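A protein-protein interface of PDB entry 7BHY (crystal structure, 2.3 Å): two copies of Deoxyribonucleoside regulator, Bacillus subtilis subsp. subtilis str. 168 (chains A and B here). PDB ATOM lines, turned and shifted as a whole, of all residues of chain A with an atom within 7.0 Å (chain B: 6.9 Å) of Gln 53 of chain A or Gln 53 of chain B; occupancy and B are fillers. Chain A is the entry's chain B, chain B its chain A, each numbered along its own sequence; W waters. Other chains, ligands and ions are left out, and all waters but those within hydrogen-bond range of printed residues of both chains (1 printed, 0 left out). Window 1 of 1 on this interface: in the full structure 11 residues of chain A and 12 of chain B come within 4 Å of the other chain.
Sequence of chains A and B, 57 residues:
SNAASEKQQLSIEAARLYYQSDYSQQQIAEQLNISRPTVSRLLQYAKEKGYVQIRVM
The backbone NH (N) of Met 57 of chain B sits at hydrogen-bond distance from the backbone carbonyl oxygen (O) of Tyr 51 of chain A (2.8 Å).
The chain-end carboxylate of Met 57 of chain B lies within hydrogen-bond range of the side-chain amide nitrogen of Gln 53 of chain A (2.8 Å).
The backbone NH (N) of Met 57 of chain A is in hydrogen-bond range of the backbone carbonyl oxygen (O) of Tyr 51 of chain B, at 3.0 Å.
The backbone carbonyl oxygen (O) of Arg 55 of chain B sits at hydrogen-bond distance from the backbone NH (N) of Gln 53 of chain A.
The backbone NH (N) of Gln 53 of chain B sits at hydrogen-bond distance from the backbone carbonyl oxygen (O) of Arg 55 of chain A.
The backbone NH (N) of Val 52 of chain B lies within hydrogen-bond range of the backbone carbonyl oxygen (O) of Ala 46 of chain B.
The backbone NH (N) of Tyr 51 of chain A lies within hydrogen-bond range of the backbone carbonyl oxygen (O) of Ala 46 of chain A (2.7 Å).
The guanidinium group (NH2) of Arg 55 of chain A sits at hydrogen-bond distance from the side-chain amide oxygen (OE1) of Gln 53 of chain A, at 2.8 Å.
The guanidinium group (NE) of Arg 55 of chain B lies within salt-bridge range of the chain-end carboxylate (O) of Met 57 of chain B (2.8 Å).
The backbone carbonyl oxygen (O) of Ala 46 of chain A lies within hydrogen-bond range of the backbone NH (N) of Val 52 of chain A (3.1 Å).
N of Tyr 51 of chain B is in hydrogen-bond range of O of Ala 46 of chain B (2.9 Å).
Among the printed residues, merely in contact across the chains: Tyr 51 of chain A with Val 56 of chain B, Gln 53 of chain A with Ile 54 of chain B, Ile 54 of chain A with Gln 53 of chain B, Val 56 of chain A with Tyr 51 of chain B, Gln 53 of chain A with Gln 53 of chain B, Val 52 of chain A with Arg 55 of chain B, Arg 55 of chain A with Val 52 of chain B, Tyr 51 of chain A with Arg 55 of chain B and Arg 55 of chain A with Tyr 51 of chain B.
Ala 46 of chain A touches none of the printed residues of chain B.
Of the printed residues of chain B, Tyr 51 of chain A touches Arg 55 (3.9 Å), Val 56 (3.3 Å) and Met 57 (2.8 Å).
Printed residues of chain B within 4 Å of Gln 53 of chain A: Gln 53 (3.6 Å), Ile 54 (3.5 Å), Arg 55 (2.8 Å) and Met 57 (2.8 Å).
Of the printed residues of chain B, Ile 54 of chain A touches Gln 53 (3.5 Å).
Of the printed residues of chain B, Arg 55 of chain A touches Tyr 51, Val 52 and Gln 53.
Of the printed residues of chain B, Val 56 of chain A touches Tyr 51.
Of chain A, only Gln 53, Ile 54 and Arg 55 come within 4 Å of Gln 53 of chain B.
Of the printed residues of chain A, Met 57 of chain B touches Tyr 51 (2.8 Å) and Gln 53 (2.8 Å).
The nearest residue of chain A that does not touch Gln 53 of chain B is Val 56 of chain A (5.3 Å).
The nearest printed residue of chain A that does not touch Val 52 of chain B is Ile 54 of chain A (4.02 Å).
Hydrophobic or aromatic side chains of chain B within 4 Å of the printed part of chain A: Val 56 and Met 57.
Along chain B the printed residues that touch a printed residue of chain A span positions 51 to 57.
Of the 10 printed residues of chain A, 7 touch a printed residue of chain B.
Printed residues of chain A that touch a printed residue of chain B: Tyr 51, Val 52, Gln 53, Ile 54, Arg 55, Val 56 and Met 57.
Tyr 51 of chain A touches Arg 55 of chain B, and with the chains exchanged Arg 55 of chain A touches Tyr 51 of chain B.
Tyr 51 of chain A touches Val 56 of chain B, and with the chains exchanged Val 56 of chain A touches Tyr 51 of chain B.
Gln 53 of chain A touches its own counterpart, Gln 53 of chain B.
Gln 53 of chain A touches Met 57 of chain B, but with the chains exchanged Met 57 of chain A does not touch Gln 53 of chain B (6.5 Å).
Of the 14 pairs that touch across the chains among the printed residues, 13 have their exchanged pair printed and touching as well.
Water W1 lies within hydrogen-bond range of NH1 of Arg 55 of chain A (2.8 Å), O of Gln 53 of chain B (3.0 Å) and O of Gln 53 of chain A (3.3 Å).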
ATOM      1  N   ALA A  46      24.429   5.078   2.278  1.00  0.00           N
ATOM      2  CA  ALA A  46      24.263   3.671   2.683  1.00  0.00           C
ATOM      3  C   ALA A  46      24.591   2.731   1.516  1.00  0.00           C
ATOM      4  O   ALA A  46      25.212   1.655   1.771  1.00  0.00           O
ATOM      5  CB  ALA A  46      22.861   3.465   3.165  1.00  0.00           C
ATOM      6  N   LYS A  47      24.139   3.080   0.305  1.00  0.00           N
ATOM      7  CA  LYS A  47      24.348   2.234  -0.896  1.00  0.00           C
ATOM      8  C   LYS A  47      25.820   2.302  -1.306  1.00  0.00           C
ATOM      9  O   LYS A  47      26.404   1.268  -1.633  1.00  0.00           O
ATOM     10  CB  LYS A  47      23.488   2.690  -2.070  1.00  0.00           C
ATOM     11  CG  LYS A  47      23.496   1.730  -3.250  1.00  0.00           C
ATOM     12  CD  LYS A  47      22.594   2.194  -4.372  1.00  0.00           C
ATOM     13  CE  LYS A  47      22.715   1.347  -5.617  1.00  0.00           C
ATOM     14  NZ  LYS A  47      21.944   1.945  -6.728  1.00  0.00           N
ATOM     15  N   GLY A  50      27.884   0.222   0.809  1.00  0.00           N
ATOM     16  CA  GLY A  50      27.347  -1.149   0.722  1.00  0.00           C
ATOM     17  C   GLY A  50      26.652  -1.616   1.996  1.00  0.00           C
ATOM     18  O   GLY A  50      26.583  -2.842   2.190  1.00  0.00           O
ATOM     19  N   TYR A  51      26.109  -0.693   2.799  1.00  0.00           N
ATOM     20  CA  TYR A  51      25.181  -1.003   3.918  1.00  0.00           C
ATOM     21  C   TYR A  51      23.853  -1.453   3.308  1.00  0.00           C
ATOM     22  O   TYR A  51      23.117  -2.265   3.874  1.00  0.00           O
ATOM     23  CB  TYR A  51      25.009   0.203   4.836  1.00  0.00           C
ATOM     24  CG  TYR A  51      26.280   0.792   5.418  1.00  0.00           C
ATOM     25  CD1 TYR A  51      27.360  -0.005   5.778  1.00  0.00           C
ATOM     26  CD2 TYR A  51      26.382   2.159   5.681  1.00  0.00           C
ATOM     27  CE1 TYR A  51      28.517   0.527   6.326  1.00  0.00           C
ATOM     28  CE2 TYR A  51      27.521   2.708   6.261  1.00  0.00           C
ATOM     29  CZ  TYR A  51      28.598   1.889   6.571  1.00  0.00           C
ATOM     30  OH  TYR A  51      29.723   2.405   7.140  1.00  0.00           O
ATOM     31  N   VAL A  52      23.547  -0.900   2.147  1.00  0.00           N
ATOM     32  CA  VAL A  52      22.443  -1.364   1.265  1.00  0.00           C
ATOM     33  C   VAL A  52      23.041  -2.074   0.046  1.00  0.00           C
ATOM     34  O   VAL A  52      23.762  -1.412  -0.697  1.00  0.00           O
ATOM     35  CB  VAL A  52      21.594  -0.162   0.810  1.00  0.00           C
ATOM     36  CG1 VAL A  52      20.478  -0.585  -0.130  1.00  0.00           C
ATOM     37  CG2 VAL A  52      21.037   0.586   1.999  1.00  0.00           C
ATOM     38  N   GLN A  53      22.654  -3.329  -0.197  1.00  0.00           N
ATOM     39  CA  GLN A  53      23.159  -4.155  -1.322  1.00  0.00           C
ATOM     40  C   GLN A  53      22.015  -4.436  -2.289  1.00  0.00           C
ATOM     41  O   GLN A  53      21.043  -5.054  -1.865  1.00  0.00           O
ATOM     42  CB  GLN A  53      23.730  -5.458  -0.775  1.00  0.00           C
ATOM     43  CG  GLN A  53      24.708  -5.264   0.380  1.00  0.00           C
ATOM     44  CD  GLN A  53      24.580  -6.369   1.409  1.00  0.00           C
ATOM     45  OE1 GLN A  53      24.869  -7.534   1.111  1.00  0.00           O
ATOM     46  NE2 GLN A  53      24.129  -6.020   2.622  1.00  0.00           N
ATOM     47  N   ILE A  54      22.172  -4.086  -3.562  1.00  0.00           N
ATOM     48  CA  ILE A  54      21.167  -4.407  -4.616  1.00  0.00           C
ATOM     49  C   ILE A  54      21.756  -5.352  -5.680  1.00  0.00           C
ATOM     50  O   ILE A  54      22.729  -5.005  -6.351  1.00  0.00           O
ATOM     51  CB  ILE A  54      20.610  -3.111  -5.205  1.00  0.00           C
ATOM     52  CG1 ILE A  54      20.180  -2.192  -4.059  1.00  0.00           C
ATOM     53  CG2 ILE A  54      19.461  -3.414  -6.171  1.00  0.00           C
ATOM     54  CD1 ILE A  54      19.525  -0.900  -4.510  1.00  0.00           C
ATOM     55  N   ARG A  55      21.133  -6.507  -5.859  1.00  0.00           N
ATOM     56  CA  ARG A  55      21.604  -7.541  -6.779  1.00  0.00           C
ATOM     57  C   ARG A  55      20.446  -7.937  -7.687  1.00  0.00           C
ATOM     58  O   ARG A  55      19.325  -8.098  -7.157  1.00  0.00           O
ATOM     59  CB  ARG A  55      22.103  -8.720  -5.952  1.00  0.00           C
ATOM     60  CG  ARG A  55      23.378  -8.403  -5.201  1.00  0.00           C
ATOM     61  CD  ARG A  55      23.574  -9.439  -4.141  1.00  0.00           C
ATOM     62  NE  ARG A  55      24.719  -9.183  -3.285  1.00  0.00           N
ATOM     63  CZ  ARG A  55      24.637  -8.932  -1.994  1.00  0.00           C
ATOM     64  NH1 ARG A  55      23.453  -8.827  -1.414  1.00  0.00           N
ATOM     65  NH2 ARG A  55      25.736  -8.750  -1.281  1.00  0.00           N
ATOM     66  N   VAL A  56      20.724  -8.134  -8.982  1.00  0.00           N
ATOM     67  CA  VAL A  56      19.688  -8.329 -10.037  1.00  0.00           C
ATOM     68  C   VAL A  56      19.961  -9.653 -10.753  1.00  0.00           C
ATOM     69  O   VAL A  56      21.132 -10.007 -10.870  1.00  0.00           O
ATOM     70  CB  VAL A  56      19.655  -7.161 -11.044  1.00  0.00           C
ATOM     71  CG1 VAL A  56      18.477  -7.250 -11.990  1.00  0.00           C
ATOM     72  CG2 VAL A  56      19.668  -5.810 -10.378  1.00  0.00           C
ATOM     73  N   MET A  57      18.907 -10.350 -11.176  1.00  0.00           N
ATOM     74  CA  MET A  57      18.984 -11.593 -11.988  1.00  0.00           C
ATOM     75  C   MET A  57      19.181 -11.208 -13.455  1.00  0.00           C
ATOM     76  O   MET A  57      19.461 -12.086 -14.311  1.00  0.00           O
ATOM     77  CB  MET A  57      17.710 -12.434 -11.888  1.00  0.00           C
ATOM     78  CG  MET A  57      17.572 -13.176 -10.551  1.00  0.00           C
ATOM     79  SD  MET A  57      16.242 -14.430 -10.524  1.00  0.00           S
ATOM     80  CE  MET A  57      16.052 -14.729 -12.282  1.00  0.00           C
ATOM     81  OXT MET A  57      19.043 -10.001 -13.764  1.00  0.00           O
ATOM     82  N   ALA B  46       9.421  -6.855 -10.419  1.00  0.00           N
ATOM     83  CA  ALA B  46      10.720  -7.545 -10.316  1.00  0.00           C
ATOM     84  C   ALA B  46      11.028  -7.697  -8.833  1.00  0.00           C
ATOM     85  O   ALA B  46      11.498  -8.737  -8.439  1.00  0.00           O
ATOM     86  CB  ALA B  46      11.789  -6.768 -11.028  1.00  0.00           C
ATOM     87  N   LYS B  47      10.737  -6.671  -8.046  1.00  0.00           N
ATOM     88  CA  LYS B  47      10.959  -6.773  -6.593  1.00  0.00           C
ATOM     89  C   LYS B  47      10.019  -7.830  -6.012  1.00  0.00           C
ATOM     90  O   LYS B  47      10.481  -8.618  -5.224  1.00  0.00           O
ATOM     91  CB  LYS B  47      10.779  -5.412  -5.929  1.00  0.00           C
ATOM     92  CG  LYS B  47      11.325  -5.329  -4.518  1.00  0.00           C
ATOM     93  CD  LYS B  47      11.876  -3.971  -4.197  1.00  0.00           C
ATOM     94  CE  LYS B  47      11.287  -3.342  -2.953  1.00  0.00           C
ATOM     95  NZ  LYS B  47      11.481  -1.871  -2.949  1.00  0.00           N
ATOM     96  N   LYS B  49       8.831 -10.538  -7.311  1.00  0.00           N
ATOM     97  CA  LYS B  49       9.233 -11.914  -7.721  1.00  0.00           C
ATOM     98  C   LYS B  49      10.646 -12.264  -7.263  1.00  0.00           C
ATOM     99  O   LYS B  49      10.978 -13.434  -7.336  1.00  0.00           O
ATOM    100  CB  LYS B  49       9.214 -12.044  -9.232  1.00  0.00           C
ATOM    101  CG  LYS B  49       7.849 -11.824  -9.841  1.00  0.00           C
ATOM    102  CD  LYS B  49       6.868 -12.845  -9.360  1.00  0.00           C
ATOM    103  CE  LYS B  49       6.402 -13.746 -10.477  1.00  0.00           C
ATOM    104  NZ  LYS B  49       5.338 -14.671 -10.029  1.00  0.00           N
ATOM    105  N   GLY B  50      11.433 -11.305  -6.772  1.00  0.00           N
ATOM    106  CA  GLY B  50      12.787 -11.586  -6.258  1.00  0.00           C
ATOM    107  C   GLY B  50      13.781 -11.504  -7.392  1.00  0.00           C
ATOM    108  O   GLY B  50      14.936 -11.914  -7.209  1.00  0.00           O
ATOM    109  N   TYR B  51      13.364 -10.991  -8.550  1.00  0.00           N
ATOM    110  CA  TYR B  51      14.324 -10.747  -9.653  1.00  0.00           C
ATOM    111  C   TYR B  51      15.301  -9.682  -9.156  1.00  0.00           C
ATOM    112  O   TYR B  51      16.511  -9.755  -9.443  1.00  0.00           O
ATOM    113  CB  TYR B  51      13.621 -10.358 -10.954  1.00  0.00           C
ATOM    114  CG  TYR B  51      12.595 -11.359 -11.424  1.00  0.00           C
ATOM    115  CD1 TYR B  51      12.584 -12.657 -10.936  1.00  0.00           C
ATOM    116  CD2 TYR B  51      11.637 -11.020 -12.378  1.00  0.00           C
ATOM    117  CE1 TYR B  51      11.632 -13.584 -11.346  1.00  0.00           C
ATOM    118  CE2 TYR B  51      10.700 -11.948 -12.831  1.00  0.00           C
ATOM    119  CZ  TYR B  51      10.693 -13.236 -12.310  1.00  0.00           C
ATOM    120  OH  TYR B  51       9.758 -14.152 -12.720  1.00  0.00           O
ATOM    121  N   VAL B  52      14.812  -8.745  -8.362  1.00  0.00           N
ATOM    122  CA  VAL B  52      15.674  -7.751  -7.666  1.00  0.00           C
ATOM    123  C   VAL B  52      15.652  -8.093  -6.190  1.00  0.00           C
ATOM    124  O   VAL B  52      14.599  -8.390  -5.732  1.00  0.00           O
ATOM    125  CB  VAL B  52      15.117  -6.341  -7.844  1.00  0.00           C
ATOM    126  CG1 VAL B  52      16.104  -5.286  -7.359  1.00  0.00           C
ATOM    127  CG2 VAL B  52      14.709  -6.128  -9.281  1.00  0.00           C
ATOM    128  N   GLN B  53      16.773  -8.031  -5.501  1.00  0.00           N
ATOM    129  CA  GLN B  53      16.834  -8.284  -4.047  1.00  0.00           C
ATOM    130  C   GLN B  53      17.633  -7.149  -3.434  1.00  0.00           C
ATOM    131  O   GLN B  53      18.754  -6.884  -3.911  1.00  0.00           O
ATOM    132  CB  GLN B  53      17.461  -9.626  -3.687  1.00  0.00           C
ATOM    133  CG  GLN B  53      16.556 -10.819  -3.989  1.00  0.00           C
ATOM    134  CD  GLN B  53      17.155 -12.139  -3.537  1.00  0.00           C
ATOM    135  OE1 GLN B  53      18.227 -12.215  -2.933  1.00  0.00           O
ATOM    136  NE2 GLN B  53      16.424 -13.209  -3.772  1.00  0.00           N
ATOM    137  N   ILE B  54      17.012  -6.488  -2.457  1.00  0.00           N
ATOM    138  CA  ILE B  54      17.606  -5.396  -1.647  1.00  0.00           C
ATOM    139  C   ILE B  54      17.798  -5.881  -0.214  1.00  0.00           C
ATOM    140  O   ILE B  54      16.850  -6.253   0.416  1.00  0.00           O
ATOM    141  CB  ILE B  54      16.714  -4.159  -1.708  1.00  0.00           C
ATOM    142  CG1 ILE B  54      16.570  -3.727  -3.173  1.00  0.00           C
ATOM    143  CG2 ILE B  54      17.303  -3.074  -0.824  1.00  0.00           C
ATOM    144  CD1 ILE B  54      15.523  -2.678  -3.397  1.00  0.00           C
ATOM    145  N   ARG B  55      19.010  -5.847   0.276  1.00  0.00           N
ATOM    146  CA  ARG B  55      19.301  -6.313   1.635  1.00  0.00           C
ATOM    147  C   ARG B  55      20.087  -5.209   2.327  1.00  0.00           C
ATOM    148  O   ARG B  55      20.951  -4.607   1.680  1.00  0.00           O
ATOM    149  CB  ARG B  55      20.086  -7.613   1.549  1.00  0.00           C
ATOM    150  CG  ARG B  55      20.373  -8.202   2.909  1.00  0.00           C
ATOM    151  CD  ARG B  55      21.472  -9.209   2.821  1.00  0.00           C
ATOM    152  NE  ARG B  55      22.006  -9.374   4.160  1.00  0.00           N
ATOM    153  CZ  ARG B  55      21.498 -10.202   5.050  1.00  0.00           C
ATOM    154  NH1 ARG B  55      20.461 -10.967   4.723  1.00  0.00           N
ATOM    155  NH2 ARG B  55      22.053 -10.273   6.251  1.00  0.00           N
ATOM    156  N   VAL B  56      19.742  -4.954   3.582  1.00  0.00           N
ATOM    157  CA  VAL B  56      20.407  -3.971   4.473  1.00  0.00           C
ATOM    158  C   VAL B  56      21.254  -4.761   5.468  1.00  0.00           C
ATOM    159  O   VAL B  56      20.704  -5.647   6.145  1.00  0.00           O
ATOM    160  CB  VAL B  56      19.365  -3.092   5.191  1.00  0.00           C
ATOM    161  CG1 VAL B  56      20.039  -2.025   6.036  1.00  0.00           C
ATOM    162  CG2 VAL B  56      18.370  -2.444   4.229  1.00  0.00           C
ATOM    163  N   MET B  57      22.548  -4.460   5.511  1.00  0.00           N
ATOM    164  CA  MET B  57      23.521  -5.113   6.415  1.00  0.00           C
ATOM    165  C   MET B  57      23.474  -6.634   6.225  1.00  0.00           C
ATOM    166  O   MET B  57      23.303  -7.089   5.082  1.00  0.00           O
ATOM    167  CB  MET B  57      23.222  -4.718   7.865  1.00  0.00           C
ATOM    168  CG  MET B  57      23.492  -3.245   8.102  1.00  0.00           C
ATOM    169  SD  MET B  57      25.030  -2.623   7.268  1.00  0.00           S
ATOM    170  CE  MET B  57      26.282  -3.080   8.479  1.00  0.00           C
ATOM    171  OXT MET B  57      23.622  -7.407   7.179  1.00  0.00           O
HETATM  172  O   HOH W   1      20.961  -8.307  -2.539  1.00  0.00           O
